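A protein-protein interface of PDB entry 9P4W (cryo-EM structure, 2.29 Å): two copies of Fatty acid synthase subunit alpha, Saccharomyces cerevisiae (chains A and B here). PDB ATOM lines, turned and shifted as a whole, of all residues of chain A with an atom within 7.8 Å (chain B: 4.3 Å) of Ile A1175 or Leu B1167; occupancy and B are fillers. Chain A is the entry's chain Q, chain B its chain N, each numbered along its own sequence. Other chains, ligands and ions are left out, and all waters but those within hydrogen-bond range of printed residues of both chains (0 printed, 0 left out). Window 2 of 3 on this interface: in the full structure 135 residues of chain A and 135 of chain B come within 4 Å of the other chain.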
ATOM      1  N   MET A1121     -18.677  34.419 -14.767  1.00  0.00           N
ATOM      2  CA  MET A1121     -17.370  34.373 -15.402  1.00  0.00           C
ATOM      3  C   MET A1121     -16.509  33.373 -14.640  1.00  0.00           C
ATOM      4  O   MET A1121     -16.916  32.840 -13.605  1.00  0.00           O
ATOM      5  CB  MET A1121     -16.717  35.760 -15.432  1.00  0.00           C
ATOM      6  CG  MET A1121     -17.499  36.792 -16.224  1.00  0.00           C
ATOM      7  SD  MET A1121     -16.548  38.279 -16.596  1.00  0.00           S
ATOM      8  CE  MET A1121     -16.061  38.796 -14.954  1.00  0.00           C
ATOM      9  N   ILE A1122     -15.311  33.108 -15.155  1.00  0.00           N
ATOM     10  CA  ILE A1122     -14.364  32.216 -14.496  1.00  0.00           C
ATOM     11  C   ILE A1122     -13.007  32.900 -14.445  1.00  0.00           C
ATOM     12  O   ILE A1122     -12.648  33.680 -15.331  1.00  0.00           O
ATOM     13  CB  ILE A1122     -14.257  30.846 -15.203  1.00  0.00           C
ATOM     14  CG1 ILE A1122     -14.022  31.024 -16.702  1.00  0.00           C
ATOM     15  CG2 ILE A1122     -15.504  30.020 -14.956  1.00  0.00           C
ATOM     16  CD1 ILE A1122     -13.562  29.762 -17.398  1.00  0.00           C
ATOM     17  N   GLN A1123     -12.253  32.606 -13.389  1.00  0.00           N
ATOM     18  CA  GLN A1123     -10.918  33.150 -13.197  1.00  0.00           C
ATOM     19  C   GLN A1123      -9.915  32.017 -13.060  1.00  0.00           C
ATOM     20  O   GLN A1123     -10.195  30.999 -12.421  1.00  0.00           O
ATOM     21  CB  GLN A1123     -10.841  34.047 -11.960  1.00  0.00           C
ATOM     22  CG  GLN A1123      -9.569  34.875 -11.910  1.00  0.00           C
ATOM     23  CD  GLN A1123      -9.480  35.747 -10.679  1.00  0.00           C
ATOM     24  OE1 GLN A1123     -10.019  36.851 -10.649  1.00  0.00           O
ATOM     25  NE2 GLN A1123      -8.787  35.261  -9.656  1.00  0.00           N
ATOM     26  N   GLU A1124      -8.744  32.207 -13.655  1.00  0.00           N
ATOM     27  CA  GLU A1124      -7.665  31.236 -13.586  1.00  0.00           C
ATOM     28  C   GLU A1124      -6.864  31.451 -12.309  1.00  0.00           C
ATOM     29  O   GLU A1124      -6.408  32.564 -12.038  1.00  0.00           O
ATOM     30  CB  GLU A1124      -6.758  31.367 -14.811  1.00  0.00           C
ATOM     31  CG  GLU A1124      -5.813  30.205 -15.018  1.00  0.00           C
ATOM     32  CD  GLU A1124      -4.704  30.526 -16.002  1.00  0.00           C
ATOM     33  OE1 GLU A1124      -4.840  31.513 -16.754  1.00  0.00           O
ATOM     34  OE2 GLU A1124      -3.692  29.795 -16.022  1.00  0.00           O
ATOM     35  N   VAL A1125      -6.699  30.386 -11.529  1.00  0.00           N
ATOM     36  CA  VAL A1125      -5.885  30.413 -10.321  1.00  0.00           C
ATOM     37  C   VAL A1125      -4.915  29.244 -10.368  1.00  0.00           C
ATOM     38  O   VAL A1125      -5.279  28.140 -10.787  1.00  0.00           O
ATOM     39  CB  VAL A1125      -6.738  30.352  -9.034  1.00  0.00           C
ATOM     40  CG1 VAL A1125      -7.874  31.360  -9.098  1.00  0.00           C
ATOM     41  CG2 VAL A1125      -7.265  28.947  -8.787  1.00  0.00           C
ATOM     42  N   ILE A1126      -3.683  29.488  -9.947  1.00  0.00           N
ATOM     43  CA  ILE A1126      -2.684  28.435  -9.826  1.00  0.00           C
ATOM     44  C   ILE A1126      -2.869  27.751  -8.480  1.00  0.00           C
ATOM     45  O   ILE A1126      -2.955  28.416  -7.441  1.00  0.00           O
ATOM     46  CB  ILE A1126      -1.262  29.000  -9.970  1.00  0.00           C
ATOM     47  CG1 ILE A1126      -1.132  29.812 -11.263  1.00  0.00           C
ATOM     48  CG2 ILE A1126      -0.244  27.873  -9.951  1.00  0.00           C
ATOM     49  CD1 ILE A1126      -1.575  29.074 -12.506  1.00  0.00           C
ATOM     50  N   VAL A1127      -2.936  26.422  -8.498  1.00  0.00           N
ATOM     51  CA  VAL A1127      -3.119  25.658  -7.271  1.00  0.00           C
ATOM     52  C   VAL A1127      -1.899  25.835  -6.377  1.00  0.00           C
ATOM     53  O   VAL A1127      -0.755  25.685  -6.823  1.00  0.00           O
ATOM     54  CB  VAL A1127      -3.358  24.175  -7.593  1.00  0.00           C
ATOM     55  CG1 VAL A1127      -3.533  23.384  -6.321  1.00  0.00           C
ATOM     56  CG2 VAL A1127      -4.575  24.018  -8.477  1.00  0.00           C
ATOM     57  N   THR A1172      -3.387  24.546 -12.984  1.00  0.00           N
ATOM     58  CA  THR A1172      -4.325  25.623 -13.261  1.00  0.00           C
ATOM     59  C   THR A1172      -5.757  25.134 -13.094  1.00  0.00           C
ATOM     60  O   THR A1172      -6.097  24.021 -13.503  1.00  0.00           O
ATOM     61  CB  THR A1172      -4.115  26.168 -14.674  1.00  0.00           C
ATOM     62  OG1 THR A1172      -2.973  27.033 -14.687  1.00  0.00           O
ATOM     63  CG2 THR A1172      -5.334  26.943 -15.148  1.00  0.00           C
ATOM     64  N   LEU A1173      -6.587  25.970 -12.474  1.00  0.00           N
ATOM     65  CA  LEU A1173      -8.013  25.714 -12.338  1.00  0.00           C
ATOM     66  C   LEU A1173      -8.776  26.961 -12.755  1.00  0.00           C
ATOM     67  O   LEU A1173      -8.191  27.993 -13.089  1.00  0.00           O
ATOM     68  CB  LEU A1173      -8.407  25.340 -10.901  1.00  0.00           C
ATOM     69  CG  LEU A1173      -8.101  23.933 -10.401  1.00  0.00           C
ATOM     70  CD1 LEU A1173      -7.986  23.942  -8.891  1.00  0.00           C
ATOM     71  CD2 LEU A1173      -9.171  22.953 -10.853  1.00  0.00           C
ATOM     72  N   TYR A1174     -10.100  26.852 -12.730  1.00  0.00           N
ATOM     73  CA  TYR A1174     -10.990  27.983 -12.945  1.00  0.00           C
ATOM     74  C   TYR A1174     -12.081  27.963 -11.887  1.00  0.00           C
ATOM     75  O   TYR A1174     -12.802  26.969 -11.754  1.00  0.00           O
ATOM     76  CB  TYR A1174     -11.599  27.947 -14.347  1.00  0.00           C
ATOM     77  CG  TYR A1174     -10.608  28.257 -15.440  1.00  0.00           C
ATOM     78  CD1 TYR A1174     -10.310  29.570 -15.776  1.00  0.00           C
ATOM     79  CD2 TYR A1174      -9.968  27.242 -16.135  1.00  0.00           C
ATOM     80  CE1 TYR A1174      -9.405  29.863 -16.773  1.00  0.00           C
ATOM     81  CE2 TYR A1174      -9.062  27.526 -17.135  1.00  0.00           C
ATOM     82  CZ  TYR A1174      -8.783  28.838 -17.447  1.00  0.00           C
ATOM     83  OH  TYR A1174      -7.881  29.128 -18.442  1.00  0.00           O
ATOM     84  N   ILE A1175     -12.197  29.048 -11.139  1.00  0.00           N
ATOM     85  CA  ILE A1175     -13.248  29.227 -10.139  1.00  0.00           C
ATOM     86  C   ILE A1175     -14.283  30.187 -10.707  1.00  0.00           C
ATOM     87  O   ILE A1175     -13.925  31.303 -11.096  1.00  0.00           O
ATOM     88  CB  ILE A1175     -12.688  29.758  -8.804  1.00  0.00           C
ATOM     89  CG1 ILE A1175     -11.819  28.693  -8.134  1.00  0.00           C
ATOM     90  CG2 ILE A1175     -13.813  30.175  -7.874  1.00  0.00           C
ATOM     91  CD1 ILE A1175     -10.364  28.881  -8.367  1.00  0.00           C
ATOM     92  N   PRO A1176     -15.555  29.801 -10.790  1.00  0.00           N
ATOM     93  CA  PRO A1176     -16.581  30.757 -11.221  1.00  0.00           C
ATOM     94  C   PRO A1176     -16.647  31.962 -10.293  1.00  0.00           C
ATOM     95  O   PRO A1176     -16.524  31.837  -9.074  1.00  0.00           O
ATOM     96  CB  PRO A1176     -17.872  29.936 -11.169  1.00  0.00           C
ATOM     97  CG  PRO A1176     -17.439  28.534 -11.317  1.00  0.00           C
ATOM     98  CD  PRO A1176     -16.099  28.438 -10.661  1.00  0.00           C
ATOM     99  N   LYS A1177     -16.843  33.138 -10.883  1.00  0.00           N
ATOM    100  CA  LYS A1177     -17.112  34.359 -10.140  1.00  0.00           C
ATOM    101  C   LYS A1177     -18.233  35.121 -10.831  1.00  0.00           C
ATOM    102  O   LYS A1177     -18.329  35.130 -12.060  1.00  0.00           O
ATOM    103  CB  LYS A1177     -15.865  35.248 -10.022  1.00  0.00           C
ATOM    104  CG  LYS A1177     -15.229  35.623 -11.346  1.00  0.00           C
ATOM    105  CD  LYS A1177     -14.020  36.519 -11.141  1.00  0.00           C
ATOM    106  CE  LYS A1177     -13.475  37.018 -12.467  1.00  0.00           C
ATOM    107  NZ  LYS A1177     -12.367  37.995 -12.295  1.00  0.00           N
ATOM    108  N   ALA A1178     -19.078  35.763 -10.033  1.00  0.00           N
ATOM    109  CA  ALA A1178     -20.252  36.458 -10.536  1.00  0.00           C
ATOM    110  C   ALA A1178     -19.977  37.951 -10.653  1.00  0.00           C
ATOM    111  O   ALA A1178     -19.248  38.533  -9.846  1.00  0.00           O
ATOM    112  CB  ALA A1178     -21.463  36.230  -9.629  1.00  0.00           C
ATOM    113  N   ASP B1130     -12.853  21.246   1.478  1.00  0.00           N
ATOM    114  CA  ASP B1130     -12.456  22.647   1.431  1.00  0.00           C
ATOM    115  C   ASP B1130     -11.107  22.796   0.738  1.00  0.00           C
ATOM    116  O   ASP B1130     -10.265  21.896   0.766  1.00  0.00           O
ATOM    117  CB  ASP B1130     -12.385  23.226   2.845  1.00  0.00           C
ATOM    118  CG  ASP B1130     -13.748  23.357   3.492  1.00  0.00           C
ATOM    119  OD1 ASP B1130     -14.676  22.630   3.086  1.00  0.00           O
ATOM    120  OD2 ASP B1130     -13.892  24.187   4.413  1.00  0.00           O
ATOM    121  N   LEU B1131     -10.905  23.923   0.076  1.00  0.00           N
ATOM    122  CA  LEU B1131      -9.650  24.185  -0.589  1.00  0.00           C
ATOM    123  C   LEU B1131      -8.800  25.049   0.294  1.00  0.00           C
ATOM    124  O   LEU B1131      -9.255  25.526   1.322  1.00  0.00           O
ATOM    125  CB  LEU B1131      -9.880  24.912  -1.906  1.00  0.00           C
ATOM    126  CG  LEU B1131     -10.176  24.061  -3.127  1.00  0.00           C
ATOM    127  CD1 LEU B1131     -11.366  23.167  -2.857  1.00  0.00           C
ATOM    128  CD2 LEU B1131     -10.442  24.957  -4.321  1.00  0.00           C
ATOM    129  N   PHE B1144     -16.387  36.425  -6.119  1.00  0.00           N
ATOM    130  CA  PHE B1144     -16.439  35.012  -5.749  1.00  0.00           C
ATOM    131  C   PHE B1144     -17.564  34.744  -4.757  1.00  0.00           C
ATOM    132  O   PHE B1144     -18.272  33.735  -4.863  1.00  0.00           O
ATOM    133  CB  PHE B1144     -15.101  34.563  -5.160  1.00  0.00           C
ATOM    134  CG  PHE B1144     -14.019  34.351  -6.179  1.00  0.00           C
ATOM    135  CD1 PHE B1144     -14.222  33.518  -7.265  1.00  0.00           C
ATOM    136  CD2 PHE B1144     -12.792  34.971  -6.042  1.00  0.00           C
ATOM    137  CE1 PHE B1144     -13.229  33.321  -8.197  1.00  0.00           C
ATOM    138  CE2 PHE B1144     -11.796  34.772  -6.973  1.00  0.00           C
ATOM    139  CZ  PHE B1144     -12.017  33.949  -8.052  1.00  0.00           C
ATOM    140  N   HIS B1148     -20.649  32.122  -5.347  1.00  0.00           N
ATOM    141  CA  HIS B1148     -20.737  30.879  -4.591  1.00  0.00           C
ATOM    142  C   HIS B1148     -21.621  30.968  -3.356  1.00  0.00           C
ATOM    143  O   HIS B1148     -22.126  29.936  -2.907  1.00  0.00           O
ATOM    144  CB  HIS B1148     -19.334  30.420  -4.181  1.00  0.00           C
ATOM    145  CG  HIS B1148     -18.443  30.112  -5.343  1.00  0.00           C
ATOM    146  ND1 HIS B1148     -18.580  28.970  -6.101  1.00  0.00           N
ATOM    147  CD2 HIS B1148     -17.411  30.800  -5.884  1.00  0.00           C
ATOM    148  CE1 HIS B1148     -17.667  28.964  -7.053  1.00  0.00           C
ATOM    149  NE2 HIS B1148     -16.945  30.063  -6.944  1.00  0.00           N
ATOM    150  N   LYS B1151     -20.966  28.657  -0.126  1.00  0.00           N
ATOM    151  CA  LYS B1151     -19.927  27.681  -0.422  1.00  0.00           C
ATOM    152  C   LYS B1151     -18.539  28.303  -0.492  1.00  0.00           C
ATOM    153  O   LYS B1151     -17.599  27.648  -0.954  1.00  0.00           O
ATOM    154  CB  LYS B1151     -20.242  26.958  -1.732  1.00  0.00           C
ATOM    155  CG  LYS B1151     -21.570  26.226  -1.735  1.00  0.00           C
ATOM    156  CD  LYS B1151     -21.452  24.870  -1.070  1.00  0.00           C
ATOM    157  CE  LYS B1151     -22.811  24.321  -0.676  1.00  0.00           C
ATOM    158  NZ  LYS B1151     -23.734  24.213  -1.839  1.00  0.00           N
ATOM    159  N   VAL B1152     -18.391  29.550  -0.055  1.00  0.00           N
ATOM    160  CA  VAL B1152     -17.097  30.216  -0.015  1.00  0.00           C
ATOM    161  C   VAL B1152     -17.069  31.139   1.194  1.00  0.00           C
ATOM    162  O   VAL B1152     -18.101  31.658   1.629  1.00  0.00           O
ATOM    163  CB  VAL B1152     -16.812  30.999  -1.319  1.00  0.00           C
ATOM    164  CG1 VAL B1152     -17.711  32.218  -1.423  1.00  0.00           C
ATOM    165  CG2 VAL B1152     -15.350  31.407  -1.392  1.00  0.00           C
ATOM    166  N   VAL B1165      -9.733  33.935   0.121  1.00  0.00           N
ATOM    167  CA  VAL B1165     -10.884  33.288  -0.471  1.00  0.00           C
ATOM    168  C   VAL B1165     -10.745  31.837  -0.144  1.00  0.00           C
ATOM    169  O   VAL B1165      -9.722  31.262  -0.409  1.00  0.00           O
ATOM    170  CB  VAL B1165     -10.987  33.537  -1.998  1.00  0.00           C
ATOM    171  CG1 VAL B1165     -12.228  32.869  -2.556  1.00  0.00           C
ATOM    172  CG2 VAL B1165     -10.998  35.023  -2.291  1.00  0.00           C
ATOM    173  N   LYS B1166     -11.771  31.256   0.437  1.00  0.00           N
ATOM    174  CA  LYS B1166     -11.734  29.879   0.817  1.00  0.00           C
ATOM    175  C   LYS B1166     -12.913  29.146   0.232  1.00  0.00           C
ATOM    176  O   LYS B1166     -14.013  29.242   0.751  1.00  0.00           O
ATOM    177  CB  LYS B1166     -11.768  29.755   2.334  1.00  0.00           C
ATOM    178  CG  LYS B1166     -11.579  28.315   2.779  1.00  0.00           C
ATOM    179  CD  LYS B1166     -11.758  28.134   4.268  1.00  0.00           C
ATOM    180  CE  LYS B1166     -11.939  26.665   4.591  1.00  0.00           C
ATOM    181  NZ  LYS B1166     -12.330  26.447   6.007  1.00  0.00           N
ATOM    182  N   LEU B1167     -12.679  28.376  -0.821  1.00  0.00           N
ATOM    183  CA  LEU B1167     -13.745  27.613  -1.455  1.00  0.00           C
ATOM    184  C   LEU B1167     -14.014  26.397  -0.618  1.00  0.00           C
ATOM    185  O   LEU B1167     -13.103  25.665  -0.297  1.00  0.00           O
ATOM    186  CB  LEU B1167     -13.396  27.240  -2.889  1.00  0.00           C
ATOM    187  CG  LEU B1167     -14.090  27.976  -4.029  1.00  0.00           C
ATOM    188  CD1 LEU B1167     -13.809  27.219  -5.312  1.00  0.00           C
ATOM    189  CD2 LEU B1167     -15.588  28.087  -3.803  1.00  0.00           C
ATOM    190  N   LEU B1168     -15.259  26.172  -0.265  1.00  0.00           N
ATOM    191  CA  LEU B1168     -15.650  25.099   0.639  1.00  0.00           C
ATOM    192  C   LEU B1168     -16.203  23.904  -0.126  1.00  0.00           C
ATOM    193  O   LEU B1168     -16.422  23.947  -1.338  1.00  0.00           O
ATOM    194  CB  LEU B1168     -16.690  25.587   1.655  1.00  0.00           C
ATOM    195  CG  LEU B1168     -16.435  26.943   2.310  1.00  0.00           C
ATOM    196  CD1 LEU B1168     -17.619  27.343   3.169  1.00  0.00           C
ATOM    197  CD2 LEU B1168     -15.162  26.917   3.132  1.00  0.00           C
ATOM    198  N   ALA B1171     -18.771  23.249  -3.539  1.00  0.00           N
ATOM    199  CA  ALA B1171     -18.695  24.300  -4.542  1.00  0.00           C
ATOM    200  C   ALA B1171     -18.296  23.726  -5.896  1.00  0.00           C
ATOM    201  O   ALA B1171     -17.872  22.574  -6.010  1.00  0.00           O
ATOM    202  CB  ALA B1171     -17.691  25.362  -4.117  1.00  0.00           C
ATOM    203  N   LEU B1173     -16.056  23.963  -9.484  1.00  0.00           N
ATOM    204  CA  LEU B1173     -14.832  24.424 -10.122  1.00  0.00           C
ATOM    205  C   LEU B1173     -14.816  23.938 -11.561  1.00  0.00           C
ATOM    206  O   LEU B1173     -15.717  23.226 -12.012  1.00  0.00           O
ATOM    207  CB  LEU B1173     -13.572  23.917  -9.406  1.00  0.00           C
ATOM    208  CG  LEU B1173     -13.151  24.587  -8.102  1.00  0.00           C
ATOM    209  CD1 LEU B1173     -12.326  23.623  -7.277  1.00  0.00           C
ATOM    210  CD2 LEU B1173     -12.373  25.863  -8.375  1.00  0.00           C
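O of Pro A1176 is in hydrogen-bond range of NE2 of His B1148.
The backbone carbonyl oxygen of Leu B1167 sits at hydrogen-bond distance from the backbone NH of Leu B1131, at 2.8 Å. N of Lys A1177 sits at hydrogen-bond distance from O of Met A1121 (2.7 Å). The backbone carbonyl oxygen (O) of Gln A1123 lies within hydrogen-bond range of the backbone NH (N) of Ile A1175 (3.1 Å). The side-chain amide oxygen of Gln A1123 sits at hydrogen-bond distance from the side-chain amino group of Lys A1177 (3.1 Å).
Among the printed residues, pairs that only touch across the chains: Ile A1175 with Leu B1173 (2.9 Å), Ile A1175 with Phe B1144 (3.2 Å), Ile A1175 with His B1148 (3.3 Å), Pro A1176 with Phe B1144 (3.4 Å), Tyr A1174 with Leu B1173 (3.6 Å), Lys A1177 with Phe B1144 (3.6 Å), Ile A1175 with Leu B1167 (3.8 Å) and Gln A1123 with Phe B1144 (3.8 Å).
Of the printed residues of chain B, Gln A1123 touches Phe B1144 (3.8 Å). Of the printed residues of chain B, Tyr A1174 touches Leu B1173 (3.6 Å). Of chain B, only Phe B1144, His B1148, Leu B1167 and Leu B1173 come within 4 Å of Ile A1175. Printed residues of chain B within 4 Å of Pro A1176: Phe B1144 (3.4 Å) and His B1148 (2.8 Å). Printed residues of chain B within 4 Å of Lys A1177: Phe B1144 (3.6 Å). Leu B1167 touches one residue of chain A. Printed residues of chain A within 4 Å of Leu B1173: Tyr A1174 and Ile A1175. The nearest printed residue of chain B that does not touch Lys A1177 is His B1148 (5.0 Å).
Of the 14 printed residues of chain A, 5 touch a printed residue of chain B. Printed residues of chain A that touch a printed residue of chain B: Gln A1123, Tyr A1174, Ile A1175, Pro A1176 and Lys A1177. Hydrophobic or aromatic side chains of chain A that line the printed part of chain B: Ile A1175 and Pro A1176. Of the 12 printed residues of chain B, 4 touch a printed residue of chain A. Hydrophobic or aromatic side chains of chain B that line the printed part of chain A: Phe B1144, His B1148, Leu B1167 and Leu B1173. Among the printed residues, 9 pairs touch across the chains.
Position printed for both chains: 1173. Of the 9 pairs that touch across the chains among the printed residues, none has its exchanged pair printed and touching as well.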
